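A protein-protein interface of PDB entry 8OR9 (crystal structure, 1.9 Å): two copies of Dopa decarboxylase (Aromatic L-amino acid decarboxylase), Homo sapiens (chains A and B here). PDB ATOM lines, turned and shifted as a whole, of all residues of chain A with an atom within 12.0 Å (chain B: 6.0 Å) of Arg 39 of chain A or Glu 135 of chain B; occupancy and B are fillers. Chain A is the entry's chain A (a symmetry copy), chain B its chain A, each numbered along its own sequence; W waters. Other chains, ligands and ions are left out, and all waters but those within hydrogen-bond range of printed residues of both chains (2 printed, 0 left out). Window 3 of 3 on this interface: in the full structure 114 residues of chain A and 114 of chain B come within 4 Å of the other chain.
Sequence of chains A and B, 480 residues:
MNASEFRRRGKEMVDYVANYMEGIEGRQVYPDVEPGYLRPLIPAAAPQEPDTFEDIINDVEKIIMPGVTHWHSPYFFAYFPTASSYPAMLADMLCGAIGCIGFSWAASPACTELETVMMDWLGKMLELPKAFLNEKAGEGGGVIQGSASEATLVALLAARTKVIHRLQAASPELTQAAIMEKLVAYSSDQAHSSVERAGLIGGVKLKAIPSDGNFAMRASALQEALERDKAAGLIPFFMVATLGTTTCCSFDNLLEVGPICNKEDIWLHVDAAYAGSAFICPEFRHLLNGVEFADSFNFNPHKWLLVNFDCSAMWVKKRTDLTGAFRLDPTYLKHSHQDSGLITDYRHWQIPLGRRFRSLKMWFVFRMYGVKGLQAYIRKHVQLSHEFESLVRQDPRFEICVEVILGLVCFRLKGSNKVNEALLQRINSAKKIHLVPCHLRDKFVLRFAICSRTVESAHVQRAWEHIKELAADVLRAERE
The side-chain carboxylate (OE1) of Glu 113 of chain B sits at hydrogen-bond distance from the backbone NH (N) of Tyr 37 of chain A (3.1 Å).
The side-chain carboxylate (OE2) of Glu 113 of chain B sits at hydrogen-bond distance from the backbone NH (N) of Gly 36 of chain A (2.7 Å).
N of Leu 38 of chain A sits at hydrogen-bond distance from OE1 of Glu 113 of chain B, 3.0 Å away.
The guanidinium group of Arg 39 of chain A sits close to the side-chain amide nitrogen of Asn 134 of chain B (3.1 Å).
The side-chain carboxylate of Asp 120 of chain B is in salt-bridge range of the guanidinium group of Arg 39 of chain A.
NZ of Lys 130 of chain B lies within salt-bridge range of OE2 of Glu 135 of chain B.
N of Glu 135 of chain B is in hydrogen-bond range of OD2 of Asp 120 of chain B (3.0 Å).
The side-chain hydroxyl (OH) of Tyr 37 of chain A is in hydrogen-bond range of the backbone carbonyl oxygen (O) of Ile 63 of chain A (2.9 Å).
The backbone NH (N) of Gly 67 of chain A lies close to the side-chain hydroxyl (OH) of Tyr 37 of chain A (3.4 Å).
The side-chain carboxylate (OD1) of Asp 120 of chain B lies within hydrogen-bond range of the backbone NH (N) of Asn 134 of chain B (2.9 Å).
Glu 113 of chain B touches Glu 34 of chain A.
Pro 35 of chain A touches Glu 113 of chain B.
Arg 39 of chain A touches Thr 116 of chain B.
Arg 39 of chain A touches Glu 135 of chain B (NH1 to CB, 3.7 Å).
CD1 of Ile 42 of chain A touches CG1 of Val 117 of chain B, 3.6 Å away.
Lys 124 of chain B touches Ala 44 of chain A.
Ala 45 of chain A touches Lys 124 of chain B (CB to CE, 3.9 Å).
Of the printed residues of chain B, Pro 35 of chain A touches Glu 113 (3.4 Å).
Of the printed residues of chain B, Gly 36 of chain A touches Glu 113 (2.7 Å).
Of the printed residues of chain B, Leu 38 of chain A touches Glu 113.
Of chain B, only Thr 116, Asp 120, Asn 134 and Glu 135 come within 4 Å of Arg 39 of chain A.
Pro 43 of chain A touches none of the printed residues of chain B.
Of the printed residues of chain B, Ala 44 of chain A touches Lys 124 (3.3 Å).
Gly 67 of chain A touches none of the printed residues of chain B.
Of the printed residues of chain A, Glu 113 of chain B touches Glu 34 (3.8 Å), Pro 35 (3.4 Å), Gly 36 (2.7 Å), Tyr 37 (3.1 Å) and Leu 38 (3.0 Å).
Printed residues of chain A within 4 Å of Thr 116 of chain B: Arg 39 (3.5 Å).
Of chain A, only Ile 42 (3.6 Å) comes within 4 Å of Val 117 of chain B.
Asp 120 of chain B touches one residue of chain A.
Glu 135 of chain B touches just one residue of chain A: Arg 39.
No residue of chain A comes within 4 Å of Lys 136 of chain B.
The nearest residue of chain A that does not touch Glu 135 of chain B is Ala 44 of chain A (4.8 Å).
Of the 20 printed residues of chain A, 9 touch a printed residue of chain B.
Hydrophobic or aromatic side chains of chain A within 4 Å of the printed part of chain B: Tyr 37, Leu 38, Ile 42 and Ala 45.
Of the 12 printed residues of chain B, 7 touch a printed residue of chain A.
Among the printed residues, Asp or Glu carboxylates within 4 Å of a Lys or Arg side-chain nitrogen of the other chain: Arg 39 of chain A with Asp 120 of chain B (2.9 Å).
No position is printed for both chains.
Of the 12 pairs that touch across the chains among the printed residues, none has its exchanged pair printed and touching as well.
Water W2 bridges OE1 of Glu 113 of chain B (2.6 Å) and N of Arg 39 of chain A (3.0 Å).
Water W1 bridges the backbone carbonyl oxygen (O) of Ala 44 of chain A (2.7 Å) and the side-chain carboxylate (OE1) of Glu 135 of chain B (3.1 Å).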
ATOM      1  N   VAL A  33     -17.506   1.758   4.761  1.00  0.00           N
ATOM      2  CA  VAL A  33     -17.588   2.060   3.336  1.00  0.00           C
ATOM      3  C   VAL A  33     -17.875   0.786   2.547  1.00  0.00           C
ATOM      4  O   VAL A  33     -17.674  -0.340   3.018  1.00  0.00           O
ATOM      5  CB  VAL A  33     -16.299   2.734   2.840  1.00  0.00           C
ATOM      6  CG1 VAL A  33     -16.033   4.021   3.609  1.00  0.00           C
ATOM      7  CG2 VAL A  33     -15.118   1.779   2.959  1.00  0.00           C
ATOM      8  N   GLU A  34     -18.349   0.977   1.323  1.00  0.00           N
ATOM      9  CA  GLU A  34     -18.582  -0.093   0.367  1.00  0.00           C
ATOM     10  C   GLU A  34     -17.600   0.022  -0.793  1.00  0.00           C
ATOM     11  O   GLU A  34     -17.011   1.086  -1.011  1.00  0.00           O
ATOM     12  CB  GLU A  34     -20.023  -0.039  -0.162  1.00  0.00           C
ATOM     13  CG  GLU A  34     -21.081  -0.333   0.894  1.00  0.00           C
ATOM     14  CD  GLU A  34     -21.083  -1.786   1.333  1.00  0.00           C
ATOM     15  OE1 GLU A  34     -20.595  -2.646   0.571  1.00  0.00           O
ATOM     16  OE2 GLU A  34     -21.577  -2.067   2.446  1.00  0.00           O
ATOM     17  N   PRO A  35     -17.378  -1.060  -1.542  1.00  0.00           N
ATOM     18  CA  PRO A  35     -16.458  -0.991  -2.685  1.00  0.00           C
ATOM     19  C   PRO A  35     -16.841   0.116  -3.656  1.00  0.00           C
ATOM     20  O   PRO A  35     -17.998   0.244  -4.058  1.00  0.00           O
ATOM     21  CB  PRO A  35     -16.595  -2.376  -3.327  1.00  0.00           C
ATOM     22  CG  PRO A  35     -16.951  -3.264  -2.195  1.00  0.00           C
ATOM     23  CD  PRO A  35     -17.837  -2.441  -1.295  1.00  0.00           C
ATOM     24  N   GLY A  36     -15.851   0.922  -4.030  1.00  0.00           N
ATOM     25  CA  GLY A  36     -16.065   2.031  -4.935  1.00  0.00           C
ATOM     26  C   GLY A  36     -16.311   3.366  -4.275  1.00  0.00           C
ATOM     27  O   GLY A  36     -16.606   4.340  -4.977  1.00  0.00           O
ATOM     28  N   TYR A  37     -16.194   3.447  -2.946  1.00  0.00           N
ATOM     29  CA  TYR A  37     -16.506   4.680  -2.231  1.00  0.00           C
ATOM     30  C   TYR A  37     -15.537   5.809  -2.561  1.00  0.00           C
ATOM     31  O   TYR A  37     -15.911   6.981  -2.454  1.00  0.00           O
ATOM     32  CB  TYR A  37     -16.499   4.430  -0.717  1.00  0.00           C
ATOM     33  CG  TYR A  37     -15.150   4.671  -0.064  1.00  0.00           C
ATOM     34  CD1 TYR A  37     -14.158   3.698  -0.095  1.00  0.00           C
ATOM     35  CD2 TYR A  37     -14.870   5.870   0.583  1.00  0.00           C
ATOM     36  CE1 TYR A  37     -12.924   3.912   0.495  1.00  0.00           C
ATOM     37  CE2 TYR A  37     -13.637   6.094   1.176  1.00  0.00           C
ATOM     38  CZ  TYR A  37     -12.668   5.111   1.129  1.00  0.00           C
ATOM     39  OH  TYR A  37     -11.440   5.324   1.714  1.00  0.00           O
ATOM     40  N   LEU A  38     -14.306   5.486  -2.965  1.00  0.00           N
ATOM     41  CA  LEU A  38     -13.244   6.486  -2.974  1.00  0.00           C
ATOM     42  C   LEU A  38     -13.268   7.362  -4.223  1.00  0.00           C
ATOM     43  O   LEU A  38     -13.093   8.582  -4.123  1.00  0.00           O
ATOM     44  CB  LEU A  38     -11.886   5.799  -2.840  1.00  0.00           C
ATOM     45  CG  LEU A  38     -10.696   6.743  -2.696  1.00  0.00           C
ATOM     46  CD1 LEU A  38     -11.037   7.788  -1.684  1.00  0.00           C
ATOM     47  CD2 LEU A  38      -9.477   5.988  -2.243  1.00  0.00           C
ATOM     48  N   ARG A  39     -13.460   6.762  -5.398  1.00  0.00           N
ATOM     49  CA  ARG A  39     -13.358   7.517  -6.645  1.00  0.00           C
ATOM     50  C   ARG A  39     -14.232   8.768  -6.700  1.00  0.00           C
ATOM     51  O   ARG A  39     -13.727   9.812  -7.151  1.00  0.00           O
ATOM     52  CB  ARG A  39     -13.662   6.597  -7.839  1.00  0.00           C
ATOM     53  CG  ARG A  39     -13.288   7.208  -9.187  1.00  0.00           C
ATOM     54  CD  ARG A  39     -13.650   6.296 -10.350  1.00  0.00           C
ATOM     55  NE  ARG A  39     -12.802   5.107 -10.405  1.00  0.00           N
ATOM     56  CZ  ARG A  39     -11.612   5.063 -10.998  1.00  0.00           C
ATOM     57  NH1 ARG A  39     -11.120   6.145 -11.589  1.00  0.00           N
ATOM     58  NH2 ARG A  39     -10.912   3.936 -11.001  1.00  0.00           N
ATOM     59  N   PRO A  40     -15.504   8.761  -6.280  1.00  0.00           N
ATOM     60  CA  PRO A  40     -16.295  10.005  -6.325  1.00  0.00           C
ATOM     61  C   PRO A  40     -15.779  11.104  -5.411  1.00  0.00           C
ATOM     62  O   PRO A  40     -16.183  12.260  -5.585  1.00  0.00           O
ATOM     63  CB  PRO A  40     -17.699   9.552  -5.897  1.00  0.00           C
ATOM     64  CG  PRO A  40     -17.722   8.085  -6.149  1.00  0.00           C
ATOM     65  CD  PRO A  40     -16.334   7.615  -5.864  1.00  0.00           C
ATOM     66  N   LEU A  41     -14.899  10.794  -4.458  1.00  0.00           N
ATOM     67  CA  LEU A  41     -14.485  11.753  -3.443  1.00  0.00           C
ATOM     68  C   LEU A  41     -13.197  12.496  -3.783  1.00  0.00           C
ATOM     69  O   LEU A  41     -12.832  13.425  -3.054  1.00  0.00           O
ATOM     70  CB  LEU A  41     -14.322  11.047  -2.090  1.00  0.00           C
ATOM     71  CG  LEU A  41     -15.569  10.298  -1.611  1.00  0.00           C
ATOM     72  CD1 LEU A  41     -15.326   9.587  -0.279  1.00  0.00           C
ATOM     73  CD2 LEU A  41     -16.751  11.249  -1.508  1.00  0.00           C
ATOM     74  N   ILE A  42     -12.500  12.115  -4.847  1.00  0.00           N
ATOM     75  CA  ILE A  42     -11.295  12.832  -5.263  1.00  0.00           C
ATOM     76  C   ILE A  42     -11.391  13.112  -6.757  1.00  0.00           C
ATOM     77  O   ILE A  42     -12.137  12.437  -7.482  1.00  0.00           O
ATOM     78  CB  ILE A  42     -10.007  12.046  -4.912  1.00  0.00           C
ATOM     79  CG1 ILE A  42      -9.961  10.704  -5.639  1.00  0.00           C
ATOM     80  CG2 ILE A  42      -9.877  11.859  -3.404  1.00  0.00           C
ATOM     81  CD1 ILE A  42      -8.764   9.863  -5.249  1.00  0.00           C
ATOM     82  N   PRO A  43     -10.663  14.120  -7.247  1.00  0.00           N
ATOM     83  CA  PRO A  43     -10.773  14.490  -8.664  1.00  0.00           C
ATOM     84  C   PRO A  43     -10.374  13.356  -9.599  1.00  0.00           C
ATOM     85  O   PRO A  43      -9.665  12.418  -9.229  1.00  0.00           O
ATOM     86  CB  PRO A  43      -9.816  15.678  -8.796  1.00  0.00           C
ATOM     87  CG  PRO A  43      -9.761  16.265  -7.429  1.00  0.00           C
ATOM     88  CD  PRO A  43      -9.849  15.091  -6.492  1.00  0.00           C
ATOM     89  N   ALA A  44     -10.842  13.466 -10.843  1.00  0.00           N
ATOM     90  CA  ALA A  44     -10.574  12.457 -11.857  1.00  0.00           C
ATOM     91  C   ALA A  44      -9.189  12.587 -12.476  1.00  0.00           C
ATOM     92  O   ALA A  44      -8.749  11.657 -13.162  1.00  0.00           O
ATOM     93  CB  ALA A  44     -11.635  12.525 -12.960  1.00  0.00           C
ATOM     94  N   ALA A  45      -8.495  13.700 -12.254  1.00  0.00           N
ATOM     95  CA  ALA A  45      -7.181  13.919 -12.839  1.00  0.00           C
ATOM     96  C   ALA A  45      -6.269  14.573 -11.811  1.00  0.00           C
ATOM     97  O   ALA A  45      -6.726  15.249 -10.886  1.00  0.00           O
ATOM     98  CB  ALA A  45      -7.262  14.786 -14.104  1.00  0.00           C
ATOM     99  N   ALA A  46      -4.967  14.361 -11.988  1.00  0.00           N
ATOM    100  CA  ALA A  46      -3.984  14.968 -11.107  1.00  0.00           C
ATOM    101  C   ALA A  46      -4.020  16.490 -11.235  1.00  0.00           C
ATOM    102  O   ALA A  46      -4.352  17.026 -12.297  1.00  0.00           O
ATOM    103  CB  ALA A  46      -2.586  14.448 -11.435  1.00  0.00           C
ATOM    104  N   ASP A  59      -7.535  15.579   3.690  1.00  0.00           N
ATOM    105  CA  ASP A  59      -8.112  14.490   2.906  1.00  0.00           C
ATOM    106  C   ASP A  59      -7.789  13.127   3.507  1.00  0.00           C
ATOM    107  O   ASP A  59      -8.588  12.191   3.377  1.00  0.00           O
ATOM    108  CB  ASP A  59      -7.622  14.557   1.460  1.00  0.00           C
ATOM    109  CG  ASP A  59      -8.343  15.615   0.646  1.00  0.00           C
ATOM    110  OD1 ASP A  59      -9.418  16.074   1.082  1.00  0.00           O
ATOM    111  OD2 ASP A  59      -7.835  15.980  -0.435  1.00  0.00           O
ATOM    112  N   LYS A  62     -10.409  12.889   6.196  1.00  0.00           N
ATOM    113  CA  LYS A  62     -11.794  12.939   5.743  1.00  0.00           C
ATOM    114  C   LYS A  62     -12.149  11.797   4.805  1.00  0.00           C
ATOM    115  O   LYS A  62     -13.309  11.372   4.763  1.00  0.00           O
ATOM    116  CB  LYS A  62     -12.068  14.270   5.041  1.00  0.00           C
ATOM    117  CG  LYS A  62     -12.000  15.484   5.944  1.00  0.00           C
ATOM    118  CD  LYS A  62     -13.383  16.019   6.244  1.00  0.00           C
ATOM    119  CE  LYS A  62     -13.463  16.551   7.664  1.00  0.00           C
ATOM    120  NZ  LYS A  62     -14.848  16.465   8.198  1.00  0.00           N
ATOM    121  N   ILE A  63     -11.179  11.287   4.053  1.00  0.00           N
ATOM    122  CA  ILE A  63     -11.480  10.483   2.877  1.00  0.00           C
ATOM    123  C   ILE A  63     -10.742   9.150   2.925  1.00  0.00           C
ATOM    124  O   ILE A  63     -11.281   8.113   2.521  1.00  0.00           O
ATOM    125  CB  ILE A  63     -11.141  11.290   1.609  1.00  0.00           C
ATOM    126  CG1 ILE A  63     -12.197  12.372   1.367  1.00  0.00           C
ATOM    127  CG2 ILE A  63     -11.036  10.403   0.412  1.00  0.00           C
ATOM    128  CD1 ILE A  63     -11.900  13.246   0.166  1.00  0.00           C
ATOM    129  N   ILE A  64      -9.510   9.160   3.435  1.00  0.00           N
ATOM    130  CA  ILE A  64      -8.731   7.927   3.505  1.00  0.00           C
ATOM    131  C   ILE A  64      -9.102   7.121   4.745  1.00  0.00           C
ATOM    132  O   ILE A  64      -9.408   5.927   4.656  1.00  0.00           O
ATOM    133  CB  ILE A  64      -7.224   8.244   3.471  1.00  0.00           C
ATOM    134  CG1 ILE A  64      -6.850   8.954   2.165  1.00  0.00           C
ATOM    135  CG2 ILE A  64      -6.408   6.969   3.655  1.00  0.00           C
ATOM    136  CD1 ILE A  64      -7.127   8.137   0.916  1.00  0.00           C
ATOM    137  N   PRO A  66     -11.784   6.846   6.665  1.00  0.00           N
ATOM    138  CA  PRO A  66     -13.032   6.059   6.653  1.00  0.00           C
ATOM    139  C   PRO A  66     -12.915   4.729   5.927  1.00  0.00           C
ATOM    140  O   PRO A  66     -13.697   3.817   6.215  1.00  0.00           O
ATOM    141  CB  PRO A  66     -14.026   6.992   5.950  1.00  0.00           C
ATOM    142  CG  PRO A  66     -13.525   8.352   6.261  1.00  0.00           C
ATOM    143  CD  PRO A  66     -12.026   8.237   6.238  1.00  0.00           C
ATOM    144  N   GLY A  67     -11.968   4.584   5.003  1.00  0.00           N
ATOM    145  CA  GLY A  67     -11.802   3.330   4.296  1.00  0.00           C
ATOM    146  C   GLY A  67     -10.608   2.525   4.768  1.00  0.00           C
ATOM    147  O   GLY A  67     -10.093   1.678   4.032  1.00  0.00           O
ATOM    148  N   GLU B 113      -8.432   1.117  -3.284  1.00  0.00           N
ATOM    149  CA  GLU B 113      -9.188   2.068  -4.095  1.00  0.00           C
ATOM    150  C   GLU B 113      -8.343   3.272  -4.496  1.00  0.00           C
ATOM    151  O   GLU B 113      -8.479   3.784  -5.613  1.00  0.00           O
ATOM    152  CB  GLU B 113     -10.441   2.512  -3.345  1.00  0.00           C
ATOM    153  CG  GLU B 113     -11.334   1.355  -2.932  1.00  0.00           C
ATOM    154  CD  GLU B 113     -12.807   1.691  -2.999  1.00  0.00           C
ATOM    155  OE1 GLU B 113     -13.151   2.806  -3.445  1.00  0.00           O
ATOM    156  OE2 GLU B 113     -13.620   0.832  -2.600  1.00  0.00           O
ATOM    157  N   THR B 116      -6.055   2.282  -7.500  1.00  0.00           N
ATOM    158  CA  THR B 116      -6.710   2.250  -8.803  1.00  0.00           C
ATOM    159  C   THR B 116      -6.902   3.656  -9.361  1.00  0.00           C
ATOM    160  O   THR B 116      -6.702   3.887 -10.559  1.00  0.00           O
ATOM    161  CB  THR B 116      -8.052   1.524  -8.693  1.00  0.00           C
ATOM    162  OG1 THR B 116      -7.845   0.221  -8.133  1.00  0.00           O
ATOM    163  CG2 THR B 116      -8.692   1.380 -10.061  1.00  0.00           C
ATOM    164  N   VAL B 117      -7.278   4.611  -8.508  1.00  0.00           N
ATOM    165  CA  VAL B 117      -7.474   5.981  -8.978  1.00  0.00           C
ATOM    166  C   VAL B 117      -6.139   6.616  -9.348  1.00  0.00           C
ATOM    167  O   VAL B 117      -6.042   7.355 -10.336  1.00  0.00           O
ATOM    168  CB  VAL B 117      -8.222   6.814  -7.922  1.00  0.00           C
ATOM    169  CG1 VAL B 117      -8.387   8.247  -8.407  1.00  0.00           C
ATOM    170  CG2 VAL B 117      -9.579   6.195  -7.616  1.00  0.00           C
ATOM    171  N   ASP B 120      -5.117   5.602 -12.704  1.00  0.00           N
ATOM    172  CA  ASP B 120      -5.842   6.350 -13.728  1.00  0.00           C
ATOM    173  C   ASP B 120      -5.289   7.761 -13.876  1.00  0.00           C
ATOM    174  O   ASP B 120      -5.159   8.262 -15.000  1.00  0.00           O
ATOM    175  CB  ASP B 120      -7.335   6.391 -13.400  1.00  0.00           C
ATOM    176  CG  ASP B 120      -8.036   5.086 -13.719  1.00  0.00           C
ATOM    177  OD1 ASP B 120      -7.488   4.295 -14.516  1.00  0.00           O
ATOM    178  OD2 ASP B 120      -9.135   4.849 -13.176  1.00  0.00           O
ATOM    179  N   LYS B 124      -3.599   8.911 -17.372  1.00  0.00           N
ATOM    180  CA  LYS B 124      -4.037  10.100 -18.094  1.00  0.00           C
ATOM    181  C   LYS B 124      -2.898  11.096 -18.278  1.00  0.00           C
ATOM    182  O   LYS B 124      -2.851  11.796 -19.295  1.00  0.00           O
ATOM    183  CB  LYS B 124      -5.215  10.750 -17.367  1.00  0.00           C
ATOM    184  CG  LYS B 124      -6.495   9.926 -17.428  1.00  0.00           C
ATOM    185  CD  LYS B 124      -7.434  10.255 -16.274  1.00  0.00           C
ATOM    186  CE  LYS B 124      -7.990  11.663 -16.392  1.00  0.00           C
ATOM    187  NZ  LYS B 124      -8.904  11.795 -17.559  1.00  0.00           N
ATOM    188  N   LYS B 130      -7.362   4.688 -23.794  1.00  0.00           N
ATOM    189  CA  LYS B 130      -8.373   4.481 -22.763  1.00  0.00           C
ATOM    190  C   LYS B 130      -8.539   3.012 -22.396  1.00  0.00           C
ATOM    191  O   LYS B 130      -9.033   2.710 -21.304  1.00  0.00           O
ATOM    192  CB  LYS B 130      -9.714   5.060 -23.221  1.00  0.00           C
ATOM    193  CG  LYS B 130      -9.714   6.574 -23.369  1.00  0.00           C
ATOM    194  CD  LYS B 130      -9.321   7.250 -22.065  1.00  0.00           C
ATOM    195  CE  LYS B 130      -9.086   8.740 -22.254  1.00  0.00           C
ATOM    196  NZ  LYS B 130      -8.406   9.350 -21.076  1.00  0.00           N
ATOM    197  N   LEU B 133      -6.945   2.218 -18.979  1.00  0.00           N
ATOM    198  CA  LEU B 133      -7.447   2.825 -17.757  1.00  0.00           C
ATOM    199  C   LEU B 133      -8.626   2.033 -17.198  1.00  0.00           C
ATOM    200  O   LEU B 133      -9.346   1.342 -17.924  1.00  0.00           O
ATOM    201  CB  LEU B 133      -7.864   4.274 -18.009  1.00  0.00           C
ATOM    202  CG  LEU B 133      -6.857   5.120 -18.789  1.00  0.00           C
ATOM    203  CD1 LEU B 133      -7.343   6.551 -18.895  1.00  0.00           C
ATOM    204  CD2 LEU B 133      -5.480   5.057 -18.141  1.00  0.00           C
ATOM    205  N   ASN B 134      -8.812   2.144 -15.878  1.00  0.00           N
ATOM    206  CA  ASN B 134      -9.925   1.478 -15.209  1.00  0.00           C
ATOM    207  C   ASN B 134     -11.193   2.319 -15.164  1.00  0.00           C
ATOM    208  O   ASN B 134     -12.294   1.754 -15.199  1.00  0.00           O
ATOM    209  CB  ASN B 134      -9.555   1.088 -13.775  1.00  0.00           C
ATOM    210  CG  ASN B 134     -10.697   0.390 -13.064  1.00  0.00           C
ATOM    211  OD1 ASN B 134     -11.107  -0.694 -13.464  1.00  0.00           O
ATOM    212  ND2 ASN B 134     -11.243   1.027 -12.031  1.00  0.00           N
ATOM    213  N   GLU B 135     -11.060   3.644 -15.076  1.00  0.00           N
ATOM    214  CA  GLU B 135     -12.214   4.534 -15.081  1.00  0.00           C
ATOM    215  C   GLU B 135     -13.170   4.194 -16.220  1.00  0.00           C
ATOM    216  O   GLU B 135     -12.770   3.701 -17.279  1.00  0.00           O
ATOM    217  CB  GLU B 135     -11.758   5.988 -15.229  1.00  0.00           C
ATOM    218  CG  GLU B 135     -10.915   6.239 -16.475  1.00  0.00           C
ATOM    219  CD  GLU B 135     -10.882   7.705 -16.878  1.00  0.00           C
ATOM    220  OE1 GLU B 135     -11.138   8.574 -16.016  1.00  0.00           O
ATOM    221  OE2 GLU B 135     -10.614   7.986 -18.065  1.00  0.00           O
ATOM    222  N   LYS B 136     -14.451   4.453 -15.972  1.00  0.00           N
ATOM    223  CA  LYS B 136     -15.527   4.338 -16.958  1.00  0.00           C
ATOM    224  C   LYS B 136     -15.744   2.899 -17.438  1.00  0.00           C
ATOM    225  O   LYS B 136     -15.950   2.647 -18.626  1.00  0.00           O
ATOM    226  CB  LYS B 136     -15.297   5.270 -18.143  1.00  0.00           C
ATOM    227  CG  LYS B 136     -15.929   6.644 -17.991  1.00  0.00           C
ATOM    228  CD  LYS B 136     -15.060   7.538 -17.117  1.00  0.00           C
ATOM    229  CE  LYS B 136     -15.506   8.991 -17.203  1.00  0.00           C
ATOM    230  NZ  LYS B 136     -16.542   9.279 -16.184  1.00  0.00           N
ATOM    231  N   ALA B 137     -15.753   1.959 -16.493  1.00  0.00           N
ATOM    232  CA  ALA B 137     -16.118   0.555 -16.695  1.00  0.00           C
ATOM    233  C   ALA B 137     -15.277  -0.154 -17.758  1.00  0.00           C
ATOM    234  O   ALA B 137     -15.707  -1.175 -18.303  1.00  0.00           O
ATOM    235  CB  ALA B 137     -17.610   0.412 -17.033  1.00  0.00           C
ATOM    236  N   GLY B 138     -14.078   0.343 -18.065  1.00  0.00           N
ATOM    237  CA  GLY B 138     -13.251  -0.312 -19.066  1.00  0.00           C
ATOM    238  C   GLY B 138     -12.706  -1.642 -18.579  1.00  0.00           C
ATOM    239  O   GLY B 138     -12.480  -1.852 -17.386  1.00  0.00           O
HETATM  240  O   HOH W   1      -9.787   9.159 -13.256  1.00  0.00           O
HETATM  241  O   HOH W   2     -13.063   3.810  -5.887  1.00  0.00           O
